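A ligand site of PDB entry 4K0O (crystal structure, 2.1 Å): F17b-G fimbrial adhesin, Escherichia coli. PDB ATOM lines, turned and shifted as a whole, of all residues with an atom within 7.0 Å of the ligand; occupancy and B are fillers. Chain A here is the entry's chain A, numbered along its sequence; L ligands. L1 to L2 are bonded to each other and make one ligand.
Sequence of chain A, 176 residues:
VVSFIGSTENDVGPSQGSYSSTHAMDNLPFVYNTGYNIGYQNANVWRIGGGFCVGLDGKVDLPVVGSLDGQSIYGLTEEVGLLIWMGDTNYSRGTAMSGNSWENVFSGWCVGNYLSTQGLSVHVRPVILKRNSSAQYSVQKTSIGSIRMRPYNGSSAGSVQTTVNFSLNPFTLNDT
N of Gly 119 sits close to O of Ala 43, at 3.3 Å.
The side-chain hydroxyl of Thr 117 is in hydrogen-bond range of the backbone carbonyl oxygen of Ala 43 (3.2 Å).
OD1 of Asp 88 sits at hydrogen-bond distance from NE2 of Gln 118, at 3.1 Å.
NH2 of Arg 93 lies within salt-bridge range of OD2 of Asp 88.
OG1 of Thr 117 is in hydrogen-bond range of OD1 of Asn 44 (3.0 Å).
The backbone NH of Ser 116 sits at hydrogen-bond distance from the backbone carbonyl oxygen of Ile 48, at 2.9 Å.
The side-chain amide oxygen (OE1) of Gln 118 is in hydrogen-bond range of the indole nitrogen (NE1) of Trp 109 (2.9 Å).
The backbone carbonyl oxygen of Gln 118 lies within hydrogen-bond range of the backbone NH of Val 45.
Merely in contact with the ligand: Trp 109 (3.3 Å) and Tyr 114 (3.6 Å).
Of the 22 residues printed, 9 come within 4 Å of the ligand.
Along chain A the residues within 4 Å of the ligand span positions 43 to 119.
The nearest printed residue that does not touch the ligand is Arg 93 (4.03 Å).
OG1 of Thr 89 lies within hydrogen-bond range of O1 of LG2 L2 (2.7 Å).
The backbone NH of Gly 119 is in hydrogen-bond range of an oxygen (O2) of LG2 L2 (2.8 Å).
The backbone carbonyl oxygen (O) of Ala 43 sits at hydrogen-bond distance from an oxygen (O1) of LG2 L2, at 3.0 Å.
The side-chain carboxylate (OD2) of Asp 88 is in hydrogen-bond range of an oxygen (O4) of LG2 L2 (3.0 Å).
The side-chain hydroxyl of Thr 117 sits at hydrogen-bond distance from a nitrogen (N1) of LG2 L2 (3.0 Å).
The side-chain hydroxyl of Ser 116 lies within hydrogen-bond range of an oxygen (O2) of LIG L1.
The side-chain amide oxygen (OE1) of Gln 118 is in hydrogen-bond range of an oxygen (O2) of LG2 L2, 3.2 Å away.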
ATOM      1  N   ASN A  42      -3.101   2.288 -17.255  1.00  0.00           N
ATOM      2  CA  ASN A  42      -2.736   2.612 -18.624  1.00  0.00           C
ATOM      3  C   ASN A  42      -2.791   1.355 -19.472  1.00  0.00           C
ATOM      4  O   ASN A  42      -2.081   0.396 -19.205  1.00  0.00           O
ATOM      5  CB  ASN A  42      -1.341   3.228 -18.661  1.00  0.00           C
ATOM      6  CG  ASN A  42      -0.976   3.768 -20.028  1.00  0.00           C
ATOM      7  OD1 ASN A  42      -1.797   3.774 -20.954  1.00  0.00           O
ATOM      8  ND2 ASN A  42       0.252   4.244 -20.167  1.00  0.00           N
ATOM      9  N   ALA A  43      -3.640   1.372 -20.485  1.00  0.00           N
ATOM     10  CA  ALA A  43      -3.841   0.199 -21.343  1.00  0.00           C
ATOM     11  C   ALA A  43      -2.693   0.013 -22.322  1.00  0.00           C
ATOM     12  O   ALA A  43      -2.536  -1.060 -22.910  1.00  0.00           O
ATOM     13  CB  ALA A  43      -5.141   0.327 -22.091  1.00  0.00           C
ATOM     14  N   ASN A  44      -1.895   1.057 -22.497  1.00  0.00           N
ATOM     15  CA  ASN A  44      -0.881   1.069 -23.546  1.00  0.00           C
ATOM     16  C   ASN A  44       0.524   1.351 -23.015  1.00  0.00           C
ATOM     17  O   ASN A  44       1.012   2.471 -23.132  1.00  0.00           O
ATOM     18  CB  ASN A  44      -1.262   2.089 -24.615  1.00  0.00           C
ATOM     19  CG  ASN A  44      -2.675   1.895 -25.118  1.00  0.00           C
ATOM     20  OD1 ASN A  44      -3.037   0.802 -25.583  1.00  0.00           O
ATOM     21  ND2 ASN A  44      -3.493   2.929 -25.030  1.00  0.00           N
ATOM     22  N   VAL A  45       1.149   0.335 -22.442  1.00  0.00           N
ATOM     23  CA  VAL A  45       2.502   0.460 -21.916  1.00  0.00           C
ATOM     24  C   VAL A  45       3.513  -0.182 -22.848  1.00  0.00           C
ATOM     25  O   VAL A  45       4.552   0.395 -23.132  1.00  0.00           O
ATOM     26  CB  VAL A  45       2.611  -0.127 -20.497  1.00  0.00           C
ATOM     27  CG1 VAL A  45       4.026   0.035 -19.949  1.00  0.00           C
ATOM     28  CG2 VAL A  45       1.626   0.561 -19.588  1.00  0.00           C
ATOM     29  N   ILE A  48       2.613  -4.852 -28.599  1.00  0.00           N
ATOM     30  CA  ILE A  48       2.997  -6.217 -28.911  1.00  0.00           C
ATOM     31  C   ILE A  48       2.288  -6.725 -30.156  1.00  0.00           C
ATOM     32  O   ILE A  48       1.245  -6.197 -30.535  1.00  0.00           O
ATOM     33  CB  ILE A  48       2.715  -7.172 -27.728  1.00  0.00           C
ATOM     34  CG1 ILE A  48       1.246  -7.100 -27.321  1.00  0.00           C
ATOM     35  CG2 ILE A  48       3.584  -6.826 -26.532  1.00  0.00           C
ATOM     36  CD1 ILE A  48       0.880  -8.066 -26.213  1.00  0.00           C
ATOM     37  N   LEU A  56       2.684 -10.190 -16.453  1.00  0.00           N
ATOM     38  CA  LEU A  56       3.248  -9.123 -15.635  1.00  0.00           C
ATOM     39  C   LEU A  56       3.745  -9.617 -14.290  1.00  0.00           C
ATOM     40  O   LEU A  56       3.077 -10.399 -13.615  1.00  0.00           O
ATOM     41  CB  LEU A  56       2.201  -8.025 -15.408  1.00  0.00           C
ATOM     42  CG  LEU A  56       1.709  -7.254 -16.638  1.00  0.00           C
ATOM     43  CD1 LEU A  56       0.497  -6.427 -16.273  1.00  0.00           C
ATOM     44  CD2 LEU A  56       2.812  -6.364 -17.153  1.00  0.00           C
ATOM     45  N   ASP A  88      -3.205  -6.545 -14.517  1.00  0.00           N
ATOM     46  CA  ASP A  88      -3.553  -6.149 -15.878  1.00  0.00           C
ATOM     47  C   ASP A  88      -4.323  -4.831 -15.872  1.00  0.00           C
ATOM     48  O   ASP A  88      -4.743  -4.354 -14.820  1.00  0.00           O
ATOM     49  CB  ASP A  88      -4.397  -7.241 -16.527  1.00  0.00           C
ATOM     50  CG  ASP A  88      -4.474  -7.091 -18.016  1.00  0.00           C
ATOM     51  OD1 ASP A  88      -3.491  -6.601 -18.608  1.00  0.00           O
ATOM     52  OD2 ASP A  88      -5.521  -7.435 -18.598  1.00  0.00           O
ATOM     53  N   THR A  89      -4.488  -4.271 -17.066  1.00  0.00           N
ATOM     54  CA  THR A  89      -5.105  -2.961 -17.273  1.00  0.00           C
ATOM     55  C   THR A  89      -6.307  -2.688 -16.373  1.00  0.00           C
ATOM     56  O   THR A  89      -6.387  -1.646 -15.727  1.00  0.00           O
ATOM     57  CB  THR A  89      -5.569  -2.789 -18.717  1.00  0.00           C
ATOM     58  OG1 THR A  89      -4.474  -3.057 -19.604  1.00  0.00           O
ATOM     59  CG2 THR A  89      -6.081  -1.388 -18.927  1.00  0.00           C
ATOM     60  N   ASN A  90      -7.257  -3.616 -16.353  1.00  0.00           N
ATOM     61  CA  ASN A  90      -8.435  -3.456 -15.540  1.00  0.00           C
ATOM     62  C   ASN A  90      -8.099  -3.528 -14.063  1.00  0.00           C
ATOM     63  O   ASN A  90      -7.366  -4.410 -13.629  1.00  0.00           O
ATOM     64  CB  ASN A  90      -9.494  -4.507 -15.892  1.00  0.00           C
ATOM     65  CG  ASN A  90     -10.054  -4.325 -17.282  1.00  0.00           C
ATOM     66  OD1 ASN A  90      -9.961  -3.247 -17.878  1.00  0.00           O
ATOM     67  ND2 ASN A  90     -10.662  -5.387 -17.818  1.00  0.00           N
ATOM     68  N   ARG A  93      -8.745  -6.651 -12.307  1.00  0.00           N
ATOM     69  CA  ARG A  93      -7.787  -7.710 -12.548  1.00  0.00           C
ATOM     70  C   ARG A  93      -6.603  -7.601 -11.596  1.00  0.00           C
ATOM     71  O   ARG A  93      -5.626  -8.333 -11.733  1.00  0.00           O
ATOM     72  CB  ARG A  93      -7.266  -7.632 -13.982  1.00  0.00           C
ATOM     73  CG  ARG A  93      -8.333  -7.694 -15.059  1.00  0.00           C
ATOM     74  CD  ARG A  93      -8.622  -9.117 -15.485  1.00  0.00           C
ATOM     75  NE  ARG A  93      -9.220  -9.189 -16.819  1.00  0.00           N
ATOM     76  CZ  ARG A  93      -8.521  -9.317 -17.944  1.00  0.00           C
ATOM     77  NH1 ARG A  93      -9.146  -9.383 -19.111  1.00  0.00           N
ATOM     78  NH2 ARG A  93      -7.198  -9.404 -17.898  1.00  0.00           N
ATOM     79  N   PHE A 106      -0.099 -10.948 -13.324  1.00  0.00           N
ATOM     80  CA  PHE A 106      -0.936 -11.228 -14.479  1.00  0.00           C
ATOM     81  C   PHE A 106      -0.389 -12.438 -15.218  1.00  0.00           C
ATOM     82  O   PHE A 106       0.698 -12.371 -15.792  1.00  0.00           O
ATOM     83  CB  PHE A 106      -0.988 -10.012 -15.411  1.00  0.00           C
ATOM     84  CG  PHE A 106      -1.700 -10.270 -16.708  1.00  0.00           C
ATOM     85  CD1 PHE A 106      -2.958 -10.861 -16.722  1.00  0.00           C
ATOM     86  CD2 PHE A 106      -1.121  -9.904 -17.907  1.00  0.00           C
ATOM     87  CE1 PHE A 106      -3.610 -11.100 -17.930  1.00  0.00           C
ATOM     88  CE2 PHE A 106      -1.779 -10.125 -19.101  1.00  0.00           C
ATOM     89  CZ  PHE A 106      -3.021 -10.732 -19.119  1.00  0.00           C
ATOM     90  N   GLY A 108      -0.976 -13.775 -17.963  1.00  0.00           N
ATOM     91  CA  GLY A 108      -0.561 -13.409 -19.298  1.00  0.00           C
ATOM     92  C   GLY A 108      -1.498 -13.795 -20.423  1.00  0.00           C
ATOM     93  O   GLY A 108      -2.605 -14.304 -20.200  1.00  0.00           O
ATOM     94  N   TRP A 109      -1.050 -13.541 -21.650  1.00  0.00           N
ATOM     95  CA  TRP A 109      -1.797 -13.843 -22.860  1.00  0.00           C
ATOM     96  C   TRP A 109      -0.888 -13.667 -24.060  1.00  0.00           C
ATOM     97  O   TRP A 109       0.211 -13.129 -23.958  1.00  0.00           O
ATOM     98  CB  TRP A 109      -3.001 -12.915 -23.009  1.00  0.00           C
ATOM     99  CG  TRP A 109      -2.632 -11.510 -23.405  1.00  0.00           C
ATOM    100  CD1 TRP A 109      -1.894 -10.622 -22.682  1.00  0.00           C
ATOM    101  CD2 TRP A 109      -3.019 -10.828 -24.612  1.00  0.00           C
ATOM    102  NE1 TRP A 109      -1.790  -9.432 -23.370  1.00  0.00           N
ATOM    103  CE2 TRP A 109      -2.476  -9.537 -24.548  1.00  0.00           C
ATOM    104  CE3 TRP A 109      -3.774 -11.186 -25.730  1.00  0.00           C
ATOM    105  CZ2 TRP A 109      -2.656  -8.604 -25.563  1.00  0.00           C
ATOM    106  CZ3 TRP A 109      -3.950 -10.264 -26.738  1.00  0.00           C
ATOM    107  CH2 TRP A 109      -3.405  -8.979 -26.644  1.00  0.00           C
ATOM    108  N   CYS A 110      -1.363 -14.107 -25.214  1.00  0.00           N
ATOM    109  CA  CYS A 110      -0.587 -14.007 -26.425  1.00  0.00           C
ATOM    110  C   CYS A 110      -1.402 -13.325 -27.505  1.00  0.00           C
ATOM    111  O   CYS A 110      -2.589 -13.617 -27.682  1.00  0.00           O
ATOM    112  CB  CYS A 110      -0.156 -15.400 -26.871  1.00  0.00           C
ATOM    113  SG  CYS A 110       0.282 -16.455 -25.476  1.00  0.00           S
ATOM    114  N   VAL A 111      -0.763 -12.403 -28.220  1.00  0.00           N
ATOM    115  CA  VAL A 111      -1.402 -11.783 -29.382  1.00  0.00           C
ATOM    116  C   VAL A 111      -1.423 -12.802 -30.505  1.00  0.00           C
ATOM    117  O   VAL A 111      -0.504 -13.610 -30.630  1.00  0.00           O
ATOM    118  CB  VAL A 111      -0.641 -10.546 -29.884  1.00  0.00           C
ATOM    119  CG1 VAL A 111      -1.048  -9.308 -29.113  1.00  0.00           C
ATOM    120  CG2 VAL A 111       0.858 -10.768 -29.791  1.00  0.00           C
ATOM    121  N   TYR A 114      -1.743 -10.148 -35.192  1.00  0.00           N
ATOM    122  CA  TYR A 114      -2.153  -8.759 -35.344  1.00  0.00           C
ATOM    123  C   TYR A 114      -1.446  -7.928 -34.281  1.00  0.00           C
ATOM    124  O   TYR A 114      -0.710  -8.468 -33.462  1.00  0.00           O
ATOM    125  CB  TYR A 114      -3.675  -8.629 -35.218  1.00  0.00           C
ATOM    126  CG  TYR A 114      -4.223  -9.071 -33.884  1.00  0.00           C
ATOM    127  CD1 TYR A 114      -4.328 -10.421 -33.576  1.00  0.00           C
ATOM    128  CD2 TYR A 114      -4.632  -8.144 -32.938  1.00  0.00           C
ATOM    129  CE1 TYR A 114      -4.829 -10.829 -32.364  1.00  0.00           C
ATOM    130  CE2 TYR A 114      -5.132  -8.554 -31.716  1.00  0.00           C
ATOM    131  CZ  TYR A 114      -5.231  -9.895 -31.438  1.00  0.00           C
ATOM    132  OH  TYR A 114      -5.729 -10.313 -30.228  1.00  0.00           O
ATOM    133  N   LEU A 115      -1.656  -6.612 -34.295  1.00  0.00           N
ATOM    134  CA  LEU A 115      -0.993  -5.754 -33.324  1.00  0.00           C
ATOM    135  C   LEU A 115      -1.944  -5.269 -32.235  1.00  0.00           C
ATOM    136  O   LEU A 115      -3.090  -4.889 -32.498  1.00  0.00           O
ATOM    137  CB  LEU A 115      -0.330  -4.561 -34.009  1.00  0.00           C
ATOM    138  CG  LEU A 115       0.933  -4.876 -34.821  1.00  0.00           C
ATOM    139  CD1 LEU A 115       1.335  -3.675 -35.641  1.00  0.00           C
ATOM    140  CD2 LEU A 115       2.053  -5.259 -33.889  1.00  0.00           C
ATOM    141  N   SER A 116      -1.459  -5.310 -30.993  1.00  0.00           N
ATOM    142  CA  SER A 116      -2.231  -4.844 -29.844  1.00  0.00           C
ATOM    143  C   SER A 116      -1.267  -4.300 -28.804  1.00  0.00           C
ATOM    144  O   SER A 116      -0.104  -4.023 -29.108  1.00  0.00           O
ATOM    145  CB  SER A 116      -3.052  -5.992 -29.256  1.00  0.00           C
ATOM    146  OG  SER A 116      -4.032  -5.504 -28.358  1.00  0.00           O
ATOM    147  N   THR A 117      -1.737  -4.151 -27.576  1.00  0.00           N
ATOM    148  CA  THR A 117      -0.936  -3.560 -26.509  1.00  0.00           C
ATOM    149  C   THR A 117      -1.027  -4.350 -25.200  1.00  0.00           C
ATOM    150  O   THR A 117      -1.962  -5.114 -24.986  1.00  0.00           O
ATOM    151  CB  THR A 117      -1.373  -2.134 -26.210  1.00  0.00           C
ATOM    152  OG1 THR A 117      -2.784  -2.127 -25.955  1.00  0.00           O
ATOM    153  CG2 THR A 117      -1.084  -1.231 -27.394  1.00  0.00           C
ATOM    154  N   GLN A 118      -0.053  -4.131 -24.328  1.00  0.00           N
ATOM    155  CA  GLN A 118      -0.123  -4.667 -22.971  1.00  0.00           C
ATOM    156  C   GLN A 118      -0.236  -3.493 -22.009  1.00  0.00           C
ATOM    157  O   GLN A 118       0.574  -2.563 -22.054  1.00  0.00           O
ATOM    158  CB  GLN A 118       1.118  -5.497 -22.633  1.00  0.00           C
ATOM    159  CG  GLN A 118       1.161  -5.984 -21.186  1.00  0.00           C
ATOM    160  CD  GLN A 118      -0.086  -6.744 -20.784  1.00  0.00           C
ATOM    161  OE1 GLN A 118      -0.644  -7.515 -21.564  1.00  0.00           O
ATOM    162  NE2 GLN A 118      -0.521  -6.542 -19.549  1.00  0.00           N
ATOM    163  N   GLY A 119      -1.244  -3.545 -21.153  1.00  0.00           N
ATOM    164  CA  GLY A 119      -1.441  -2.492 -20.164  1.00  0.00           C
ATOM    165  C   GLY A 119      -1.290  -3.020 -18.758  1.00  0.00           C
ATOM    166  O   GLY A 119      -1.014  -4.197 -18.549  1.00  0.00           O
ATOM    167  N   LEU A 120      -1.455  -2.125 -17.784  1.00  0.00           N
ATOM    168  CA  LEU A 120      -1.323  -2.475 -16.381  1.00  0.00           C
ATOM    169  C   LEU A 120      -2.145  -1.555 -15.485  1.00  0.00           C
ATOM    170  O   LEU A 120      -2.598  -0.502 -15.925  1.00  0.00           O
ATOM    171  CB  LEU A 120       0.165  -2.448 -15.981  1.00  0.00           C
ATOM    172  CG  LEU A 120       1.032  -1.262 -16.391  1.00  0.00           C
ATOM    173  CD1 LEU A 120       0.871  -0.102 -15.437  1.00  0.00           C
ATOM    174  CD2 LEU A 120       2.486  -1.683 -16.476  1.00  0.00           C
HETATM  175  C1  LIG L   1      -8.105  -7.119 -28.490  1.00  0.00           C
HETATM  176  C2  LIG L   1      -7.792  -6.131 -27.466  1.00  0.00           C
HETATM  177  C3  LIG L   1      -6.877  -6.584 -26.434  1.00  0.00           C
HETATM  178  C4  LIG L   1      -7.034  -7.922 -25.975  1.00  0.00           C
HETATM  179  C5  LIG L   1      -7.040  -8.868 -27.157  1.00  0.00           C
HETATM  180  C6  LIG L   1      -7.224 -10.162 -26.738  1.00  0.00           C
HETATM  181  C7  LIG L   1     -10.479  -7.168 -28.728  1.00  0.00           C
HETATM  182  O1  LIG L   1      -9.246  -6.770 -29.170  1.00  0.00           O
HETATM  183  O2  LIG L   1      -7.096  -5.130 -28.203  1.00  0.00           O
HETATM  184  O3  LIG L   1      -6.924  -5.700 -25.249  1.00  0.00           O
HETATM  185  O4  LIG L   1      -8.326  -7.931 -25.522  1.00  0.00           O
HETATM  186  O5  LIG L   1      -8.205  -8.432 -27.961  1.00  0.00           O
HETATM  187  O6  LIG L   1      -8.368 -10.417 -26.041  1.00  0.00           O
HETATM  188  C1  LG2 L   2      -5.713  -5.727 -24.553  1.00  0.00           C
HETATM  189  C2  LG2 L   2      -5.514  -4.452 -23.901  1.00  0.00           C
HETATM  190  C3  LG2 L   2      -4.417  -4.433 -23.010  1.00  0.00           C
HETATM  191  C4  LG2 L   2      -4.349  -5.539 -22.068  1.00  0.00           C
HETATM  192  C5  LG2 L   2      -4.491  -6.867 -22.778  1.00  0.00           C
HETATM  193  C6  LG2 L   2      -4.687  -7.854 -21.845  1.00  0.00           C
HETATM  194  C7  LG2 L   2      -6.354  -2.597 -25.319  1.00  0.00           C
HETATM  195  C8  LG2 L   2      -7.619  -2.657 -24.612  1.00  0.00           C
HETATM  196  N1  LG2 L   2      -5.273  -3.457 -24.990  1.00  0.00           N
HETATM  197  O1  LG2 L   2      -4.494  -3.205 -22.276  1.00  0.00           O
HETATM  198  O2  LG2 L   2      -3.151  -5.532 -21.395  1.00  0.00           O
HETATM  199  O3  LG2 L   2      -5.768  -6.716 -23.544  1.00  0.00           O
HETATM  200  O4  LG2 L   2      -5.992  -8.019 -21.483  1.00  0.00           O
HETATM  201  O5  LG2 L   2      -6.209  -1.793 -26.190  1.00  0.00           O
